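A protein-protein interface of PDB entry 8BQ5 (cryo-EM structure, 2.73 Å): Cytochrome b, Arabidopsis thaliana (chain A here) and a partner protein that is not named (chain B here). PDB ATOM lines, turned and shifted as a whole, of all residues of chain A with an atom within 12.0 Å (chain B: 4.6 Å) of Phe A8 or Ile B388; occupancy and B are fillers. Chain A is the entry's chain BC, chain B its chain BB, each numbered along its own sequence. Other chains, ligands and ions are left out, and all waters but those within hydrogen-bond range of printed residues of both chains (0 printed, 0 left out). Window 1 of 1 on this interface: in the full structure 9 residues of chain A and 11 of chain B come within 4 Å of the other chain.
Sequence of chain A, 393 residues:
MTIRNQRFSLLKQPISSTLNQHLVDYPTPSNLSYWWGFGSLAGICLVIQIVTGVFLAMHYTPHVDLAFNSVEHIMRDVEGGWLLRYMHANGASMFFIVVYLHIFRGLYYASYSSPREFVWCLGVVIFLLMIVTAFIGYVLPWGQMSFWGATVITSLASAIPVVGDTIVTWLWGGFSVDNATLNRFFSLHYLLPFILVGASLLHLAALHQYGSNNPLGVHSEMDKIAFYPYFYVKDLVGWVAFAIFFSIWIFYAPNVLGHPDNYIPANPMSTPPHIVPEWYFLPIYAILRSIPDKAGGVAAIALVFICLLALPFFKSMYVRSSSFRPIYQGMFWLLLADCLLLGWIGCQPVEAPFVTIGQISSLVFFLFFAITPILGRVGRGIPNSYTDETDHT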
ATOM      1  N   THR A   2     -15.162 -18.222   0.385  1.00  0.00           N
ATOM      2  CA  THR A   2     -15.318 -19.663   0.713  1.00  0.00           C
ATOM      3  C   THR A   2     -16.269 -19.850   1.898  1.00  0.00           C
ATOM      4  O   THR A   2     -15.918 -19.396   3.002  1.00  0.00           O
ATOM      5  CB  THR A   2     -13.969 -20.321   1.032  1.00  0.00           C
ATOM      6  OG1 THR A   2     -13.123 -20.226  -0.115  1.00  0.00           O
ATOM      7  CG2 THR A   2     -14.103 -21.772   1.444  1.00  0.00           C
ATOM      8  N   ILE A   3     -17.436 -20.461   1.677  1.00  0.00           N
ATOM      9  CA  ILE A   3     -18.339 -20.812   2.814  1.00  0.00           C
ATOM     10  C   ILE A   3     -18.122 -22.305   3.056  1.00  0.00           C
ATOM     11  O   ILE A   3     -18.391 -23.080   2.133  1.00  0.00           O
ATOM     12  CB  ILE A   3     -19.816 -20.487   2.503  1.00  0.00           C
ATOM     13  CG1 ILE A   3     -19.979 -19.126   1.819  1.00  0.00           C
ATOM     14  CG2 ILE A   3     -20.661 -20.584   3.763  1.00  0.00           C
ATOM     15  CD1 ILE A   3     -19.620 -17.948   2.695  1.00  0.00           C
ATOM     16  N   ARG A   4     -17.637 -22.696   4.233  1.00  0.00           N
ATOM     17  CA  ARG A   4     -17.288 -24.124   4.472  1.00  0.00           C
ATOM     18  C   ARG A   4     -18.544 -24.921   4.832  1.00  0.00           C
ATOM     19  O   ARG A   4     -18.700 -25.274   6.012  1.00  0.00           O
ATOM     20  CB  ARG A   4     -16.193 -24.216   5.539  1.00  0.00           C
ATOM     21  CG  ARG A   4     -14.978 -23.356   5.227  1.00  0.00           C
ATOM     22  CD  ARG A   4     -13.893 -23.397   6.285  1.00  0.00           C
ATOM     23  NE  ARG A   4     -12.852 -22.420   6.000  1.00  0.00           N
ATOM     24  CZ  ARG A   4     -11.758 -22.660   5.283  1.00  0.00           C
ATOM     25  NH1 ARG A   4     -11.546 -23.861   4.772  1.00  0.00           N
ATOM     26  NH2 ARG A   4     -10.877 -21.697   5.083  1.00  0.00           N
ATOM     27  N   ASN A   5     -19.391 -25.201   3.839  1.00  0.00           N
ATOM     28  CA  ASN A   5     -20.635 -25.980   4.062  1.00  0.00           C
ATOM     29  C   ASN A   5     -20.296 -27.464   3.945  1.00  0.00           C
ATOM     30  O   ASN A   5     -20.740 -28.234   4.801  1.00  0.00           O
ATOM     31  CB  ASN A   5     -21.733 -25.560   3.083  1.00  0.00           C
ATOM     32  CG  ASN A   5     -22.136 -24.108   3.225  1.00  0.00           C
ATOM     33  OD1 ASN A   5     -22.386 -23.431   2.232  1.00  0.00           O
ATOM     34  ND2 ASN A   5     -22.197 -23.620   4.453  1.00  0.00           N
ATOM     35  N   GLN A   6     -19.508 -27.829   2.934  1.00  0.00           N
ATOM     36  CA  GLN A   6     -19.099 -29.242   2.740  1.00  0.00           C
ATOM     37  C   GLN A   6     -17.701 -29.470   3.320  1.00  0.00           C
ATOM     38  O   GLN A   6     -17.026 -28.480   3.650  1.00  0.00           O
ATOM     39  CB  GLN A   6     -19.123 -29.597   1.255  1.00  0.00           C
ATOM     40  CG  GLN A   6     -20.519 -29.635   0.657  1.00  0.00           C
ATOM     41  CD  GLN A   6     -20.469 -29.888  -0.828  1.00  0.00           C
ATOM     42  OE1 GLN A   6     -19.546 -29.468  -1.519  1.00  0.00           O
ATOM     43  NE2 GLN A   6     -21.472 -30.580  -1.335  1.00  0.00           N
ATOM     44  N   ARG A   7     -17.288 -30.734   3.428  1.00  0.00           N
ATOM     45  CA  ARG A   7     -15.948 -31.080   3.956  1.00  0.00           C
ATOM     46  C   ARG A   7     -14.950 -31.194   2.808  1.00  0.00           C
ATOM     47  O   ARG A   7     -15.169 -32.044   1.927  1.00  0.00           O
ATOM     48  CB  ARG A   7     -15.988 -32.381   4.761  1.00  0.00           C
ATOM     49  CG  ARG A   7     -16.675 -32.258   6.111  1.00  0.00           C
ATOM     50  CD  ARG A   7     -16.374 -33.478   6.953  1.00  0.00           C
ATOM     51  NE  ARG A   7     -16.719 -34.733   6.303  1.00  0.00           N
ATOM     52  CZ  ARG A   7     -17.808 -35.449   6.557  1.00  0.00           C
ATOM     53  NH1 ARG A   7     -18.686 -35.039   7.455  1.00  0.00           N
ATOM     54  NH2 ARG A   7     -18.020 -36.579   5.908  1.00  0.00           N
ATOM     55  N   PHE A   8     -13.922 -30.354   2.804  1.00  0.00           N
ATOM     56  CA  PHE A   8     -12.822 -30.392   1.853  1.00  0.00           C
ATOM     57  C   PHE A   8     -11.760 -31.357   2.384  1.00  0.00           C
ATOM     58  O   PHE A   8     -12.064 -32.221   3.212  1.00  0.00           O
ATOM     59  CB  PHE A   8     -12.309 -28.975   1.595  1.00  0.00           C
ATOM     60  CG  PHE A   8     -13.200 -28.175   0.692  1.00  0.00           C
ATOM     61  CD1 PHE A   8     -13.035 -28.220  -0.682  1.00  0.00           C
ATOM     62  CD2 PHE A   8     -14.218 -27.398   1.215  1.00  0.00           C
ATOM     63  CE1 PHE A   8     -13.861 -27.494  -1.515  1.00  0.00           C
ATOM     64  CE2 PHE A   8     -15.047 -26.669   0.386  1.00  0.00           C
ATOM     65  CZ  PHE A   8     -14.868 -26.718  -0.980  1.00  0.00           C
ATOM     66  N   SER A   9     -10.535 -31.264   1.868  1.00  0.00           N
ATOM     67  CA  SER A   9      -9.430 -32.139   2.252  1.00  0.00           C
ATOM     68  C   SER A   9      -9.414 -32.421   3.750  1.00  0.00           C
ATOM     69  O   SER A   9      -9.603 -31.521   4.571  1.00  0.00           O
ATOM     70  CB  SER A   9      -8.102 -31.506   1.831  1.00  0.00           C
ATOM     71  OG  SER A   9      -7.024 -32.033   2.581  1.00  0.00           O
ATOM     72  N   LEU A  10      -9.188 -33.693   4.092  1.00  0.00           N
ATOM     73  CA  LEU A  10      -9.290 -34.141   5.478  1.00  0.00           C
ATOM     74  C   LEU A  10      -8.257 -33.469   6.376  1.00  0.00           C
ATOM     75  O   LEU A  10      -8.450 -33.395   7.594  1.00  0.00           O
ATOM     76  CB  LEU A  10      -9.149 -35.666   5.530  1.00  0.00           C
ATOM     77  CG  LEU A  10      -9.425 -36.456   6.814  1.00  0.00           C
ATOM     78  CD1 LEU A  10      -8.159 -36.627   7.649  1.00  0.00           C
ATOM     79  CD2 LEU A  10     -10.539 -35.816   7.634  1.00  0.00           C
ATOM     80  N   LEU A  11      -7.161 -32.971   5.802  1.00  0.00           N
ATOM     81  CA  LEU A  11      -6.142 -32.317   6.617  1.00  0.00           C
ATOM     82  C   LEU A  11      -6.591 -30.956   7.131  1.00  0.00           C
ATOM     83  O   LEU A  11      -5.943 -30.403   8.025  1.00  0.00           O
ATOM     84  CB  LEU A  11      -4.842 -32.171   5.825  1.00  0.00           C
ATOM     85  CG  LEU A  11      -4.122 -33.471   5.467  1.00  0.00           C
ATOM     86  CD1 LEU A  11      -3.280 -33.283   4.220  1.00  0.00           C
ATOM     87  CD2 LEU A  11      -3.265 -33.939   6.631  1.00  0.00           C
ATOM     88  N   LYS A  12      -7.672 -30.400   6.593  1.00  0.00           N
ATOM     89  CA  LYS A  12      -8.181 -29.114   7.050  1.00  0.00           C
ATOM     90  C   LYS A  12      -9.337 -29.241   8.033  1.00  0.00           C
ATOM     91  O   LYS A  12      -9.852 -28.216   8.493  1.00  0.00           O
ATOM     92  CB  LYS A  12      -8.617 -28.263   5.856  1.00  0.00           C
ATOM     93  CG  LYS A  12      -7.485 -27.869   4.933  1.00  0.00           C
ATOM     94  CD  LYS A  12      -7.388 -26.362   4.825  1.00  0.00           C
ATOM     95  CE  LYS A  12      -6.808 -25.951   3.497  1.00  0.00           C
ATOM     96  NZ  LYS A  12      -7.854 -25.458   2.551  1.00  0.00           N
ATOM     97  N   GLN A  13      -9.759 -30.455   8.358  1.00  0.00           N
ATOM     98  CA  GLN A  13     -10.801 -30.651   9.349  1.00  0.00           C
ATOM     99  C   GLN A  13     -10.266 -30.329  10.741  1.00  0.00           C
ATOM    100  O   GLN A  13      -9.055 -30.339  10.967  1.00  0.00           O
ATOM    101  CB  GLN A  13     -11.313 -32.086   9.292  1.00  0.00           C
ATOM    102  CG  GLN A  13     -12.248 -32.356   8.128  1.00  0.00           C
ATOM    103  CD  GLN A  13     -13.343 -31.317   8.014  1.00  0.00           C
ATOM    104  OE1 GLN A  13     -14.239 -31.251   8.851  1.00  0.00           O
ATOM    105  NE2 GLN A  13     -13.271 -30.493   6.976  1.00  0.00           N
ATOM    106  N   PRO A  14     -11.153 -30.027  11.695  1.00  0.00           N
ATOM    107  CA  PRO A  14     -10.685 -29.737  13.061  1.00  0.00           C
ATOM    108  C   PRO A  14      -9.906 -30.874  13.695  1.00  0.00           C
ATOM    109  O   PRO A  14      -9.111 -30.623  14.609  1.00  0.00           O
ATOM    110  CB  PRO A  14     -11.986 -29.459  13.825  1.00  0.00           C
ATOM    111  CG  PRO A  14     -12.940 -29.004  12.787  1.00  0.00           C
ATOM    112  CD  PRO A  14     -12.594 -29.757  11.537  1.00  0.00           C
ATOM    113  N   ILE A  15     -10.106 -32.115  13.244  1.00  0.00           N
ATOM    114  CA  ILE A  15      -9.385 -33.247  13.814  1.00  0.00           C
ATOM    115  C   ILE A  15      -7.886 -33.134  13.555  1.00  0.00           C
ATOM    116  O   ILE A  15      -7.074 -33.587  14.369  1.00  0.00           O
ATOM    117  CB  ILE A  15      -9.962 -34.568  13.266  1.00  0.00           C
ATOM    118  CG1 ILE A  15      -9.340 -35.772  13.975  1.00  0.00           C
ATOM    119  CG2 ILE A  15      -9.759 -34.665  11.761  1.00  0.00           C
ATOM    120  CD1 ILE A  15      -9.506 -35.752  15.475  1.00  0.00           C
ATOM    121  N   SER A  16      -7.488 -32.526  12.433  1.00  0.00           N
ATOM    122  CA  SER A  16      -6.074 -32.449  12.092  1.00  0.00           C
ATOM    123  C   SER A  16      -5.654 -31.077  11.578  1.00  0.00           C
ATOM    124  O   SER A  16      -4.592 -30.969  10.954  1.00  0.00           O
ATOM    125  CB  SER A  16      -5.718 -33.514  11.048  1.00  0.00           C
ATOM    126  OG  SER A  16      -6.503 -33.361   9.880  1.00  0.00           O
ATOM    127  N   SER A  17      -6.451 -30.031  11.809  1.00  0.00           N
ATOM    128  CA  SER A  17      -6.085 -28.704  11.324  1.00  0.00           C
ATOM    129  C   SER A  17      -4.830 -28.183  12.014  1.00  0.00           C
ATOM    130  O   SER A  17      -3.990 -27.539  11.378  1.00  0.00           O
ATOM    131  CB  SER A  17      -7.247 -27.733  11.524  1.00  0.00           C
ATOM    132  OG  SER A  17      -7.535 -27.563  12.900  1.00  0.00           O
ATOM    133  N   ASN A  20      -1.878 -29.917  10.535  1.00  0.00           N
ATOM    134  CA  ASN A  20      -1.640 -29.439   9.177  1.00  0.00           C
ATOM    135  C   ASN A  20      -0.926 -28.094   9.172  1.00  0.00           C
ATOM    136  O   ASN A  20       0.032 -27.897   8.416  1.00  0.00           O
ATOM    137  CB  ASN A  20      -2.961 -29.338   8.418  1.00  0.00           C
ATOM    138  CG  ASN A  20      -2.763 -29.202   6.925  1.00  0.00           C
ATOM    139  OD1 ASN A  20      -2.271 -30.117   6.267  1.00  0.00           O
ATOM    140  ND2 ASN A  20      -3.137 -28.051   6.382  1.00  0.00           N
ATOM    141  N   ASP A  25       1.830 -27.790   6.531  1.00  0.00           N
ATOM    142  CA  ASP A  25       1.806 -26.629   5.598  1.00  0.00           C
ATOM    143  C   ASP A  25       2.560 -25.410   6.146  1.00  0.00           C
ATOM    144  O   ASP A  25       2.469 -24.353   5.502  1.00  0.00           O
ATOM    145  CB  ASP A  25       0.367 -26.276   5.217  1.00  0.00           C
ATOM    146  CG  ASP A  25      -0.133 -27.078   4.030  1.00  0.00           C
ATOM    147  OD1 ASP A  25       0.167 -26.682   2.886  1.00  0.00           O
ATOM    148  OD2 ASP A  25      -0.810 -28.098   4.257  1.00  0.00           O
ATOM    149  N   ARG B 382     -19.730 -28.683  -5.959  1.00  0.00           N
ATOM    150  CA  ARG B 382     -18.756 -28.298  -4.942  1.00  0.00           C
ATOM    151  C   ARG B 382     -18.435 -26.812  -5.017  1.00  0.00           C
ATOM    152  O   ARG B 382     -18.309 -26.139  -3.989  1.00  0.00           O
ATOM    153  CB  ARG B 382     -17.486 -29.133  -5.097  1.00  0.00           C
ATOM    154  CG  ARG B 382     -17.461 -30.360  -4.216  1.00  0.00           C
ATOM    155  CD  ARG B 382     -16.282 -31.260  -4.529  1.00  0.00           C
ATOM    156  NE  ARG B 382     -16.616 -32.660  -4.303  1.00  0.00           N
ATOM    157  CZ  ARG B 382     -16.774 -33.208  -3.106  1.00  0.00           C
ATOM    158  NH1 ARG B 382     -16.603 -32.509  -1.996  1.00  0.00           N
ATOM    159  NH2 ARG B 382     -17.111 -34.492  -3.019  1.00  0.00           N
ATOM    160  N   VAL B 383     -18.291 -26.284  -6.233  1.00  0.00           N
ATOM    161  CA  VAL B 383     -17.960 -24.871  -6.397  1.00  0.00           C
ATOM    162  C   VAL B 383     -19.135 -23.993  -5.982  1.00  0.00           C
ATOM    163  O   VAL B 383     -18.973 -23.013  -5.247  1.00  0.00           O
ATOM    164  CB  VAL B 383     -17.528 -24.590  -7.848  1.00  0.00           C
ATOM    165  CG1 VAL B 383     -17.384 -23.100  -8.078  1.00  0.00           C
ATOM    166  CG2 VAL B 383     -16.230 -25.311  -8.161  1.00  0.00           C
ATOM    167  N   ASN B 386     -20.144 -24.062  -2.029  1.00  0.00           N
ATOM    168  CA  ASN B 386     -19.176 -23.423  -1.098  1.00  0.00           C
ATOM    169  C   ASN B 386     -18.704 -22.063  -1.622  1.00  0.00           C
ATOM    170  O   ASN B 386     -17.885 -21.445  -0.929  1.00  0.00           O
ATOM    171  CB  ASN B 386     -18.004 -24.369  -0.832  1.00  0.00           C
ATOM    172  CG  ASN B 386     -18.453 -25.724  -0.326  1.00  0.00           C
ATOM    173  OD1 ASN B 386     -18.820 -25.866   0.837  1.00  0.00           O
ATOM    174  ND2 ASN B 386     -18.430 -26.725  -1.188  1.00  0.00           N
ATOM    175  N   GLU B 387     -19.203 -21.609  -2.777  1.00  0.00           N
ATOM    176  CA  GLU B 387     -18.840 -20.318  -3.371  1.00  0.00           C
ATOM    177  C   GLU B 387     -17.328 -20.091  -3.339  1.00  0.00           C
ATOM    178  O   GLU B 387     -16.819 -19.169  -2.702  1.00  0.00           O
ATOM    179  CB  GLU B 387     -19.576 -19.161  -2.687  1.00  0.00           C
ATOM    180  CG  GLU B 387     -20.861 -19.538  -1.975  1.00  0.00           C
ATOM    181  CD  GLU B 387     -21.762 -18.342  -1.743  1.00  0.00           C
ATOM    182  OE1 GLU B 387     -21.257 -17.293  -1.289  1.00  0.00           O
ATOM    183  OE2 GLU B 387     -22.977 -18.450  -2.013  1.00  0.00           O
ATOM    184  N   ILE B 388     -16.609 -20.954  -4.052  1.00  0.00           N
ATOM    185  CA  ILE B 388     -15.155 -20.919  -4.058  1.00  0.00           C
ATOM    186  C   ILE B 388     -14.600 -20.529  -5.428  1.00  0.00           C
ATOM    187  O   ILE B 388     -13.413 -20.694  -5.681  1.00  0.00           O
ATOM    188  CB  ILE B 388     -14.568 -22.260  -3.580  1.00  0.00           C
ATOM    189  CG1 ILE B 388     -15.012 -23.394  -4.505  1.00  0.00           C
ATOM    190  CG2 ILE B 388     -14.971 -22.533  -2.143  1.00  0.00           C
ATOM    191  CD1 ILE B 388     -14.671 -24.769  -3.991  1.00  0.00           C
ATOM    192  N   ALA B 389     -15.445 -20.012  -6.318  1.00  0.00           N
ATOM    193  CA  ALA B 389     -14.971 -19.560  -7.619  1.00  0.00           C
ATOM    194  C   ALA B 389     -15.989 -18.609  -8.229  1.00  0.00           C
ATOM    195  O   ALA B 389     -17.195 -18.752  -8.019  1.00  0.00           O
ATOM    196  CB  ALA B 389     -14.715 -20.734  -8.570  1.00  0.00           C
ATOM    197  N   ALA B 411     -11.229 -17.221  -9.717  1.00  0.00           N
ATOM    198  CA  ALA B 411     -11.619 -17.142  -8.316  1.00  0.00           C
ATOM    199  C   ALA B 411     -10.791 -16.077  -7.616  1.00  0.00           C
ATOM    200  O   ALA B 411      -9.847 -15.519  -8.180  1.00  0.00           O
ATOM    201  CB  ALA B 411     -11.461 -18.494  -7.614  1.00  0.00           C
ATOM    202  N   CYS B 415      -9.813 -18.210  -2.103  1.00  0.00           N
ATOM    203  CA  CYS B 415     -10.537 -19.416  -2.475  1.00  0.00           C
ATOM    204  C   CYS B 415      -9.695 -20.393  -3.285  1.00  0.00           C
ATOM    205  O   CYS B 415     -10.190 -21.472  -3.626  1.00  0.00           O
ATOM    206  CB  CYS B 415     -11.795 -19.051  -3.273  1.00  0.00           C
ATOM    207  SG  CYS B 415     -12.962 -17.979  -2.398  1.00  0.00           S
ATOM    208  N   ASP B 418      -8.890 -24.269  -1.617  1.00  0.00           N
ATOM    209  CA  ASP B 418     -10.055 -25.194  -1.612  1.00  0.00           C
ATOM    210  C   ASP B 418     -10.510 -25.462  -3.050  1.00  0.00           C
ATOM    211  O   ASP B 418     -10.921 -26.601  -3.318  1.00  0.00           O
ATOM    212  CB  ASP B 418     -11.193 -24.669  -0.737  1.00  0.00           C
ATOM    213  CG  ASP B 418     -10.970 -24.906   0.745  1.00  0.00           C
ATOM    214  OD1 ASP B 418     -10.193 -25.820   1.080  1.00  0.00           O
ATOM    215  OD2 ASP B 418     -11.571 -24.175   1.551  1.00  0.00           O
ATOM    216  N   LEU B 419     -10.445 -24.458  -3.930  1.00  0.00           N
ATOM    217  CA  LEU B 419     -10.810 -24.666  -5.327  1.00  0.00           C
ATOM    218  C   LEU B 419      -9.861 -25.645  -6.004  1.00  0.00           C
ATOM    219  O   LEU B 419     -10.296 -26.515  -6.767  1.00  0.00           O
ATOM    220  CB  LEU B 419     -10.819 -23.334  -6.073  1.00  0.00           C
ATOM    221  CG  LEU B 419     -11.184 -23.408  -7.556  1.00  0.00           C
ATOM    222  CD1 LEU B 419     -12.546 -24.056  -7.743  1.00  0.00           C
ATOM    223  CD2 LEU B 419     -11.146 -22.031  -8.186  1.00  0.00           C
ATOM    224  N   TYR B 421      -8.103 -28.057  -4.623  1.00  0.00           N
ATOM    225  CA  TYR B 421      -8.404 -29.401  -4.145  1.00  0.00           C
ATOM    226  C   TYR B 421      -9.654 -29.953  -4.819  1.00  0.00           C
ATOM    227  O   TYR B 421      -9.683 -31.114  -5.243  1.00  0.00           O
ATOM    228  CB  TYR B 421      -8.574 -29.396  -2.624  1.00  0.00           C
ATOM    229  CG  TYR B 421      -9.182 -30.672  -2.087  1.00  0.00           C
ATOM    230  CD1 TYR B 421      -8.388 -31.770  -1.795  1.00  0.00           C
ATOM    231  CD2 TYR B 421     -10.551 -30.778  -1.877  1.00  0.00           C
ATOM    232  CE1 TYR B 421      -8.937 -32.938  -1.311  1.00  0.00           C
ATOM    233  CE2 TYR B 421     -11.108 -31.943  -1.396  1.00  0.00           C
ATOM    234  CZ  TYR B 421     -10.298 -33.018  -1.114  1.00  0.00           C
ATOM    235  OH  TYR B 421     -10.851 -34.180  -0.630  1.00  0.00           O
ATOM    236  N   ALA B 422     -10.700 -29.131  -4.921  1.00  0.00           N
ATOM    237  CA  ALA B 422     -11.963 -29.600  -5.484  1.00  0.00           C
ATOM    238  C   ALA B 422     -11.819 -29.962  -6.955  1.00  0.00           C
ATOM    239  O   ALA B 422     -12.375 -30.968  -7.411  1.00  0.00           O
ATOM    240  CB  ALA B 422     -13.047 -28.539  -5.296  1.00  0.00           C
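Hydrophobic or aromatic side chains of chain B that line the printed part of chain A: Ile B388 and Tyr B421.
The side-chain hydroxyl (OG) of Ser A9 lies close to the backbone NH (N) of Leu A11 (3.4 Å). The side-chain amide nitrogen (ND2) of Asn B386 lies within hydrogen-bond range of the backbone carbonyl oxygen (O) of Arg B382, at 2.9 Å. The backbone NH of Ile B388 sits at hydrogen-bond distance from the backbone carbonyl oxygen of Val B383.
Among the printed residues, merely in contact across the chains: Ser A9 with Tyr B421, Thr A2 with Asp B418, Gln A6 with Arg B382, Thr A2 with Asn B386, Phe A8 with Asp B418, Phe A8 with Asn B386, Thr A2 with Ile B388, Phe A8 with Ile B388, Thr A2 with Glu B387, Phe A8 with Tyr B421 and Ile A3 with Glu B387.
Of the printed residues of chain B, Phe A8 touches Asn B386, Ile B388, Asp B418 and Tyr B421. Ile B388 touches just these residues of chain A: Thr A2 and Phe A8. Asn B386 touches just these residues of chain A: Thr A2 (3.5 Å), Ile A3 (2.8 Å), Asn A5 (3.1 Å), Gln A6 (3.0 Å) and Phe A8 (3.6 Å). No residue of chain A comes within 4 Å of Ala B389. No residue of chain A comes within 4 Å of Ala B411. Of chain A, only Thr A2, Arg A4, Phe A8 and Lys A12 come within 4 Å of Asp B418. No residue of chain A comes within 4 Å of Leu B419. Tyr B421 touches just these residues of chain A: Phe A8 (3.8 Å) and Ser A9 (3.4 Å). Printed residues of chain B within 4 Å of Ile A3: Asn B386 and Glu B387. Of the printed residues of chain B, Arg A4 touches Asp B418. Leu A10 touches none of the printed residues of chain B. The nearest printed residue of chain B that does not touch Phe A8 is Ala B422 (4.01 Å). The nearest printed residue of chain B that does not touch Gln A6 is Val B383 (5.8 Å).
The side-chain sulfur of Cys B415 is in hydrogen-bond range of the side-chain hydroxyl of Thr A2, at 3.2 Å. The backbone carbonyl oxygen (O) of Asn B386 is in hydrogen-bond range of the backbone NH (N) of Ile A3, 2.8 Å away. The side-chain amino group (NZ) of Lys A12 lies within salt-bridge range of the side-chain carboxylate (OD1) of Asp B418 (2.8 Å). The side-chain amide oxygen of Asn B386 is in hydrogen-bond range of the backbone NH of Asn A5. N of Gln A6 sits at hydrogen-bond distance from OD1 of Asn B386 (3.0 Å). The side-chain carboxylate (OD2) of Asp B418 is in salt-bridge range of the guanidinium group (NH1) of Arg A4 (3.2 Å).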
